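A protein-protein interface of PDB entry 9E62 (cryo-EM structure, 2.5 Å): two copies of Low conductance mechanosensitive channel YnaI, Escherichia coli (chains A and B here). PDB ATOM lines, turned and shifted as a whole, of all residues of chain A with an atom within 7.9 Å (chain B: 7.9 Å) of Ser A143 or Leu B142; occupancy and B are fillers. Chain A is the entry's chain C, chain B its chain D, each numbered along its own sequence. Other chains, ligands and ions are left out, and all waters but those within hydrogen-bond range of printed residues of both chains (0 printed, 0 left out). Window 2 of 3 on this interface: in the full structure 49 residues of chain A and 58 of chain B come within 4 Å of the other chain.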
ATOM      1  N   MET A 140     -31.598  16.388 -11.955  1.00  0.00           N
ATOM      2  CA  MET A 140     -30.448  17.153 -12.416  1.00  0.00           C
ATOM      3  C   MET A 140     -30.301  16.887 -13.909  1.00  0.00           C
ATOM      4  O   MET A 140     -31.200  16.339 -14.556  1.00  0.00           O
ATOM      5  CB  MET A 140     -29.201  16.733 -11.626  1.00  0.00           C
ATOM      6  CG  MET A 140     -28.930  17.512 -10.356  1.00  0.00           C
ATOM      7  SD  MET A 140     -28.852  19.291 -10.519  1.00  0.00           S
ATOM      8  CE  MET A 140     -27.449  19.625  -9.448  1.00  0.00           C
ATOM      9  N   SER A 141     -29.157  17.265 -14.472  1.00  0.00           N
ATOM     10  CA  SER A 141     -28.843  16.905 -15.848  1.00  0.00           C
ATOM     11  C   SER A 141     -28.528  15.419 -15.953  1.00  0.00           C
ATOM     12  O   SER A 141     -27.710  14.893 -15.196  1.00  0.00           O
ATOM     13  CB  SER A 141     -27.656  17.729 -16.343  1.00  0.00           C
ATOM     14  OG  SER A 141     -27.142  17.201 -17.551  1.00  0.00           O
ATOM     15  N   LEU A 142     -29.144  14.750 -16.928  1.00  0.00           N
ATOM     16  CA  LEU A 142     -28.993  13.307 -17.082  1.00  0.00           C
ATOM     17  C   LEU A 142     -27.603  12.892 -17.550  1.00  0.00           C
ATOM     18  O   LEU A 142     -27.387  11.710 -17.842  1.00  0.00           O
ATOM     19  CB  LEU A 142     -30.052  12.757 -18.043  1.00  0.00           C
ATOM     20  CG  LEU A 142     -31.450  12.497 -17.475  1.00  0.00           C
ATOM     21  CD1 LEU A 142     -31.364  11.722 -16.167  1.00  0.00           C
ATOM     22  CD2 LEU A 142     -32.229  13.791 -17.287  1.00  0.00           C
ATOM     23  N   SER A 143     -26.663  13.829 -17.635  1.00  0.00           N
ATOM     24  CA  SER A 143     -25.268  13.529 -17.926  1.00  0.00           C
ATOM     25  C   SER A 143     -24.379  13.593 -16.695  1.00  0.00           C
ATOM     26  O   SER A 143     -23.411  12.834 -16.601  1.00  0.00           O
ATOM     27  CB  SER A 143     -24.731  14.492 -18.992  1.00  0.00           C
ATOM     28  OG  SER A 143     -23.316  14.511 -19.005  1.00  0.00           O
ATOM     29  N   GLY A 144     -24.678  14.488 -15.753  1.00  0.00           N
ATOM     30  CA  GLY A 144     -23.874  14.574 -14.545  1.00  0.00           C
ATOM     31  C   GLY A 144     -23.993  13.350 -13.657  1.00  0.00           C
ATOM     32  O   GLY A 144     -22.987  12.843 -13.150  1.00  0.00           O
ATOM     33  N   LEU A 145     -25.219  12.858 -13.452  1.00  0.00           N
ATOM     34  CA  LEU A 145     -25.403  11.683 -12.607  1.00  0.00           C
ATOM     35  C   LEU A 145     -24.735  10.459 -13.209  1.00  0.00           C
ATOM     36  O   LEU A 145     -24.184   9.631 -12.482  1.00  0.00           O
ATOM     37  CB  LEU A 145     -26.885  11.389 -12.353  1.00  0.00           C
ATOM     38  CG  LEU A 145     -27.822  12.375 -11.649  1.00  0.00           C
ATOM     39  CD1 LEU A 145     -27.314  12.707 -10.248  1.00  0.00           C
ATOM     40  CD2 LEU A 145     -28.075  13.621 -12.449  1.00  0.00           C
ATOM     41  N   LEU A 146     -24.786  10.318 -14.534  1.00  0.00           N
ATOM     42  CA  LEU A 146     -24.125   9.178 -15.160  1.00  0.00           C
ATOM     43  C   LEU A 146     -22.639   9.161 -14.833  1.00  0.00           C
ATOM     44  O   LEU A 146     -22.112   8.146 -14.369  1.00  0.00           O
ATOM     45  CB  LEU A 146     -24.347   9.205 -16.672  1.00  0.00           C
ATOM     46  CG  LEU A 146     -25.713   8.704 -17.143  1.00  0.00           C
ATOM     47  CD1 LEU A 146     -25.786   8.676 -18.662  1.00  0.00           C
ATOM     48  CD2 LEU A 146     -26.010   7.329 -16.562  1.00  0.00           C
ATOM     49  N   THR A 147     -21.956  10.293 -15.025  1.00  0.00           N
ATOM     50  CA  THR A 147     -20.527  10.355 -14.738  1.00  0.00           C
ATOM     51  C   THR A 147     -20.245  10.161 -13.251  1.00  0.00           C
ATOM     52  O   THR A 147     -19.336   9.410 -12.875  1.00  0.00           O
ATOM     53  CB  THR A 147     -19.956  11.689 -15.221  1.00  0.00           C
ATOM     54  OG1 THR A 147     -19.684  11.613 -16.627  1.00  0.00           O
ATOM     55  CG2 THR A 147     -18.673  12.026 -14.480  1.00  0.00           C
ATOM     56  N   PHE A 148     -21.018  10.830 -12.391  1.00  0.00           N
ATOM     57  CA  PHE A 148     -20.782  10.739 -10.953  1.00  0.00           C
ATOM     58  C   PHE A 148     -20.961   9.308 -10.459  1.00  0.00           C
ATOM     59  O   PHE A 148     -20.097   8.766  -9.755  1.00  0.00           O
ATOM     60  CB  PHE A 148     -21.729  11.687 -10.215  1.00  0.00           C
ATOM     61  CG  PHE A 148     -21.235  12.113  -8.863  1.00  0.00           C
ATOM     62  CD1 PHE A 148     -19.903  11.964  -8.518  1.00  0.00           C
ATOM     63  CD2 PHE A 148     -22.104  12.663  -7.937  1.00  0.00           C
ATOM     64  CE1 PHE A 148     -19.445  12.358  -7.276  1.00  0.00           C
ATOM     65  CE2 PHE A 148     -21.653  13.057  -6.692  1.00  0.00           C
ATOM     66  CZ  PHE A 148     -20.321  12.904  -6.361  1.00  0.00           C
ATOM     67  N   GLY A 149     -22.077   8.678 -10.830  1.00  0.00           N
ATOM     68  CA  GLY A 149     -22.320   7.311 -10.422  1.00  0.00           C
ATOM     69  C   GLY A 149     -21.328   6.337 -11.022  1.00  0.00           C
ATOM     70  O   GLY A 149     -20.937   5.368 -10.373  1.00  0.00           O
ATOM     71  N   LEU B 132     -19.994  19.676 -13.146  1.00  0.00           N
ATOM     72  CA  LEU B 132     -20.395  18.445 -13.817  1.00  0.00           C
ATOM     73  C   LEU B 132     -21.863  18.128 -13.543  1.00  0.00           C
ATOM     74  O   LEU B 132     -22.565  17.613 -14.422  1.00  0.00           O
ATOM     75  CB  LEU B 132     -19.476  17.298 -13.385  1.00  0.00           C
ATOM     76  CG  LEU B 132     -19.705  15.834 -13.795  1.00  0.00           C
ATOM     77  CD1 LEU B 132     -20.727  15.110 -12.927  1.00  0.00           C
ATOM     78  CD2 LEU B 132     -20.080  15.731 -15.270  1.00  0.00           C
ATOM     79  N   LEU B 133     -22.348  18.432 -12.336  1.00  0.00           N
ATOM     80  CA  LEU B 133     -23.751  18.185 -12.013  1.00  0.00           C
ATOM     81  C   LEU B 133     -24.667  19.227 -12.647  1.00  0.00           C
ATOM     82  O   LEU B 133     -25.781  18.902 -13.072  1.00  0.00           O
ATOM     83  CB  LEU B 133     -23.952  18.166 -10.497  1.00  0.00           C
ATOM     84  CG  LEU B 133     -24.017  16.818  -9.774  1.00  0.00           C
ATOM     85  CD1 LEU B 133     -25.413  16.222  -9.885  1.00  0.00           C
ATOM     86  CD2 LEU B 133     -22.978  15.849 -10.299  1.00  0.00           C
ATOM     87  N   GLY B 135     -24.260  21.223 -15.417  1.00  0.00           N
ATOM     88  CA  GLY B 135     -23.707  21.649 -16.685  1.00  0.00           C
ATOM     89  C   GLY B 135     -24.613  21.452 -17.881  1.00  0.00           C
ATOM     90  O   GLY B 135     -24.150  21.009 -18.936  1.00  0.00           O
ATOM     91  N   GLU B 136     -25.902  21.760 -17.742  1.00  0.00           N
ATOM     92  CA  GLU B 136     -26.810  21.718 -18.880  1.00  0.00           C
ATOM     93  C   GLU B 136     -27.667  22.967 -19.038  1.00  0.00           C
ATOM     94  O   GLU B 136     -27.998  23.321 -20.173  1.00  0.00           O
ATOM     95  CB  GLU B 136     -27.726  20.484 -18.792  1.00  0.00           C
ATOM     96  CG  GLU B 136     -28.860  20.591 -17.787  1.00  0.00           C
ATOM     97  CD  GLU B 136     -30.176  20.955 -18.444  1.00  0.00           C
ATOM     98  OE1 GLU B 136     -30.256  20.894 -19.688  1.00  0.00           O
ATOM     99  OE2 GLU B 136     -31.132  21.302 -17.718  1.00  0.00           O
ATOM    100  N   HIS B 137     -28.036  23.643 -17.947  1.00  0.00           N
ATOM    101  CA  HIS B 137     -28.832  24.861 -18.063  1.00  0.00           C
ATOM    102  C   HIS B 137     -28.033  26.007 -18.663  1.00  0.00           C
ATOM    103  O   HIS B 137     -28.542  26.714 -19.541  1.00  0.00           O
ATOM    104  CB  HIS B 137     -29.378  25.262 -16.695  1.00  0.00           C
ATOM    105  CG  HIS B 137     -30.233  24.215 -16.057  1.00  0.00           C
ATOM    106  ND1 HIS B 137     -29.705  23.126 -15.395  1.00  0.00           N
ATOM    107  CD2 HIS B 137     -31.579  24.086 -15.974  1.00  0.00           C
ATOM    108  CE1 HIS B 137     -30.687  22.375 -14.934  1.00  0.00           C
ATOM    109  NE2 HIS B 137     -31.835  22.935 -15.272  1.00  0.00           N
ATOM    110  N   GLY B 139     -24.878  24.987 -19.680  1.00  0.00           N
ATOM    111  CA  GLY B 139     -23.781  24.055 -19.830  1.00  0.00           C
ATOM    112  C   GLY B 139     -23.147  24.000 -21.198  1.00  0.00           C
ATOM    113  O   GLY B 139     -22.893  25.026 -21.842  1.00  0.00           O
ATOM    114  N   MET B 140     -22.886  22.778 -21.645  1.00  0.00           N
ATOM    115  CA  MET B 140     -21.945  22.514 -22.723  1.00  0.00           C
ATOM    116  C   MET B 140     -22.563  21.438 -23.607  1.00  0.00           C
ATOM    117  O   MET B 140     -23.752  21.122 -23.499  1.00  0.00           O
ATOM    118  CB  MET B 140     -20.596  22.078 -22.134  1.00  0.00           C
ATOM    119  CG  MET B 140     -19.611  23.190 -21.843  1.00  0.00           C
ATOM    120  SD  MET B 140     -19.238  24.293 -23.201  1.00  0.00           S
ATOM    121  CE  MET B 140     -17.464  24.458 -22.968  1.00  0.00           C
ATOM    122  N   SER B 141     -21.756  20.853 -24.488  1.00  0.00           N
ATOM    123  CA  SER B 141     -22.196  19.698 -25.258  1.00  0.00           C
ATOM    124  C   SER B 141     -22.291  18.468 -24.369  1.00  0.00           C
ATOM    125  O   SER B 141     -21.352  18.140 -23.643  1.00  0.00           O
ATOM    126  CB  SER B 141     -21.226  19.440 -26.409  1.00  0.00           C
ATOM    127  OG  SER B 141     -21.452  18.169 -26.987  1.00  0.00           O
ATOM    128  N   LEU B 142     -23.415  17.755 -24.461  1.00  0.00           N
ATOM    129  CA  LEU B 142     -23.666  16.603 -23.601  1.00  0.00           C
ATOM    130  C   LEU B 142     -22.772  15.409 -23.918  1.00  0.00           C
ATOM    131  O   LEU B 142     -22.974  14.330 -23.347  1.00  0.00           O
ATOM    132  CB  LEU B 142     -25.138  16.188 -23.678  1.00  0.00           C
ATOM    133  CG  LEU B 142     -26.136  16.975 -22.824  1.00  0.00           C
ATOM    134  CD1 LEU B 142     -25.627  17.121 -21.397  1.00  0.00           C
ATOM    135  CD2 LEU B 142     -26.442  18.336 -23.433  1.00  0.00           C
ATOM    136  N   SER B 143     -21.802  15.569 -24.812  1.00  0.00           N
ATOM    137  CA  SER B 143     -20.798  14.550 -25.086  1.00  0.00           C
ATOM    138  C   SER B 143     -19.452  14.858 -24.452  1.00  0.00           C
ATOM    139  O   SER B 143     -18.737  13.934 -24.055  1.00  0.00           O
ATOM    140  CB  SER B 143     -20.620  14.376 -26.599  1.00  0.00           C
ATOM    141  OG  SER B 143     -19.403  13.721 -26.903  1.00  0.00           O
ATOM    142  N   GLY B 144     -19.084  16.136 -24.355  1.00  0.00           N
ATOM    143  CA  GLY B 144     -17.816  16.488 -23.735  1.00  0.00           C
ATOM    144  C   GLY B 144     -17.772  16.187 -22.250  1.00  0.00           C
ATOM    145  O   GLY B 144     -16.782  15.646 -21.748  1.00  0.00           O
ATOM    146  N   LEU B 145     -18.839  16.534 -21.523  1.00  0.00           N
ATOM    147  CA  LEU B 145     -18.860  16.275 -20.086  1.00  0.00           C
ATOM    148  C   LEU B 145     -18.825  14.785 -19.793  1.00  0.00           C
ATOM    149  O   LEU B 145     -18.193  14.357 -18.825  1.00  0.00           O
ATOM    150  CB  LEU B 145     -20.083  16.904 -19.411  1.00  0.00           C
ATOM    151  CG  LEU B 145     -20.355  18.411 -19.415  1.00  0.00           C
ATOM    152  CD1 LEU B 145     -19.201  19.176 -18.773  1.00  0.00           C
ATOM    153  CD2 LEU B 145     -20.673  18.948 -20.781  1.00  0.00           C
ATOM    154  N   LEU B 146     -19.509  13.979 -20.606  1.00  0.00           N
ATOM    155  CA  LEU B 146     -19.473  12.538 -20.386  1.00  0.00           C
ATOM    156  C   LEU B 146     -18.046  12.012 -20.444  1.00  0.00           C
ATOM    157  O   LEU B 146     -17.596  11.322 -19.526  1.00  0.00           O
ATOM    158  CB  LEU B 146     -20.354  11.826 -21.411  1.00  0.00           C
ATOM    159  CG  LEU B 146     -21.856  11.859 -21.120  1.00  0.00           C
ATOM    160  CD1 LEU B 146     -22.623  11.034 -22.142  1.00  0.00           C
ATOM    161  CD2 LEU B 146     -22.138  11.368 -19.708  1.00  0.00           C
ATOM    162  N   THR B 147     -17.304  12.370 -21.495  1.00  0.00           N
ATOM    163  CA  THR B 147     -15.927  11.903 -21.624  1.00  0.00           C
ATOM    164  C   THR B 147     -15.041  12.459 -20.513  1.00  0.00           C
ATOM    165  O   THR B 147     -14.246  11.723 -19.914  1.00  0.00           O
ATOM    166  CB  THR B 147     -15.371  12.290 -22.996  1.00  0.00           C
ATOM    167  OG1 THR B 147     -15.801  11.336 -23.974  1.00  0.00           O
ATOM    168  CG2 THR B 147     -13.853  12.334 -22.970  1.00  0.00           C
ATOM    169  N   GLY B 149     -15.821  13.626 -17.442  1.00  0.00           N
ATOM    170  CA  GLY B 149     -16.136  13.021 -16.164  1.00  0.00           C
ATOM    171  C   GLY B 149     -15.767  11.554 -16.106  1.00  0.00           C
ATOM    172  O   GLY B 149     -15.339  11.059 -15.065  1.00  0.00           O
ATOM    173  N   GLY B 150     -15.925  10.834 -17.219  1.00  0.00           N
ATOM    174  CA  GLY B 150     -15.509   9.445 -17.242  1.00  0.00           C
ATOM    175  C   GLY B 150     -14.019   9.288 -17.016  1.00  0.00           C
ATOM    176  O   GLY B 150     -13.588   8.460 -16.212  1.00  0.00           O
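Ser A143 touches Leu B142, but with the chains exchanged Leu A142 does not touch Ser B143 (9.7 Å). Ser A143 touches Leu B146, but with the chains exchanged Leu A146 does not touch Ser B143 (10.0 Å). Thr A147 touches Leu B145, but with the chains exchanged Leu A145 does not touch Thr B147 (11.3 Å). Thr A147 touches Gly B149, but with the chains exchanged Gly A149 does not touch Thr B147 (12.3 Å). 9 positions are printed for both chains. Of the 10 pairs that touch across the chains among the printed residues, none has its exchanged pair printed and touching as well.
Among the printed residues, merely in contact across the chains: Thr A147 with Gly B149 (3.2 Å), Gly A144 with Leu B132 (3.2 Å), Ser A141 with Glu B136 (3.4 Å), Ser A143 with Leu B146 (3.4 Å), Thr A147 with Leu B146 (3.6 Å), Ser A143 with Leu B142 (3.7 Å), Met A140 with Leu B133 (3.8 Å), Thr A147 with Leu B145 (3.8 Å), Thr A147 with Gly B150 (3.9 Å) and Ser A141 with Leu B133 (3.9 Å).
Ser A143 touches just these residues of chain B: Leu B142 and Leu B146. Leu B142 touches just one residue of chain A: Ser A143 (3.7 Å). Of chain B, only Leu B132 comes within 4 Å of Gly A144. Of the printed residues of chain A, Leu B132 touches Gly A144 (3.2 Å). Of the printed residues of chain B, Met A140 touches Leu B133. Of the printed residues of chain A, Glu B136 touches Ser A141. Of the printed residues of chain A, Gly B150 touches Thr A147. Leu A142 touches none of the printed residues of chain B. His B137 touches none of the printed residues of chain A. The nearest residue of chain A that does not touch Leu B142 is Ser A141 (4.1 Å). The nearest printed residue of chain A that does not touch Gly B150 is Phe A148 (7.0 Å).
Printed residues of chain A that touch a printed residue of chain B: Met A140, Ser A141, Ser A143, Gly A144 and Thr A147. Hydrophobic or aromatic side chains of chain A within 4 Å of the printed part of chain B: Met A140. Printed residues of chain B that touch a printed residue of chain A: Leu B132, Leu B133, Glu B136, Leu B142, Leu B145, Leu B146, Gly B149 and Gly B150. Along chain B the printed residues that touch a printed residue of chain A span positions 132 to 150.
NE2 of His B137 sits close to OE2 of Glu B136 (3.0 Å). OG of Ser A141 sits close to N of Ser A143, 3.4 Å away.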
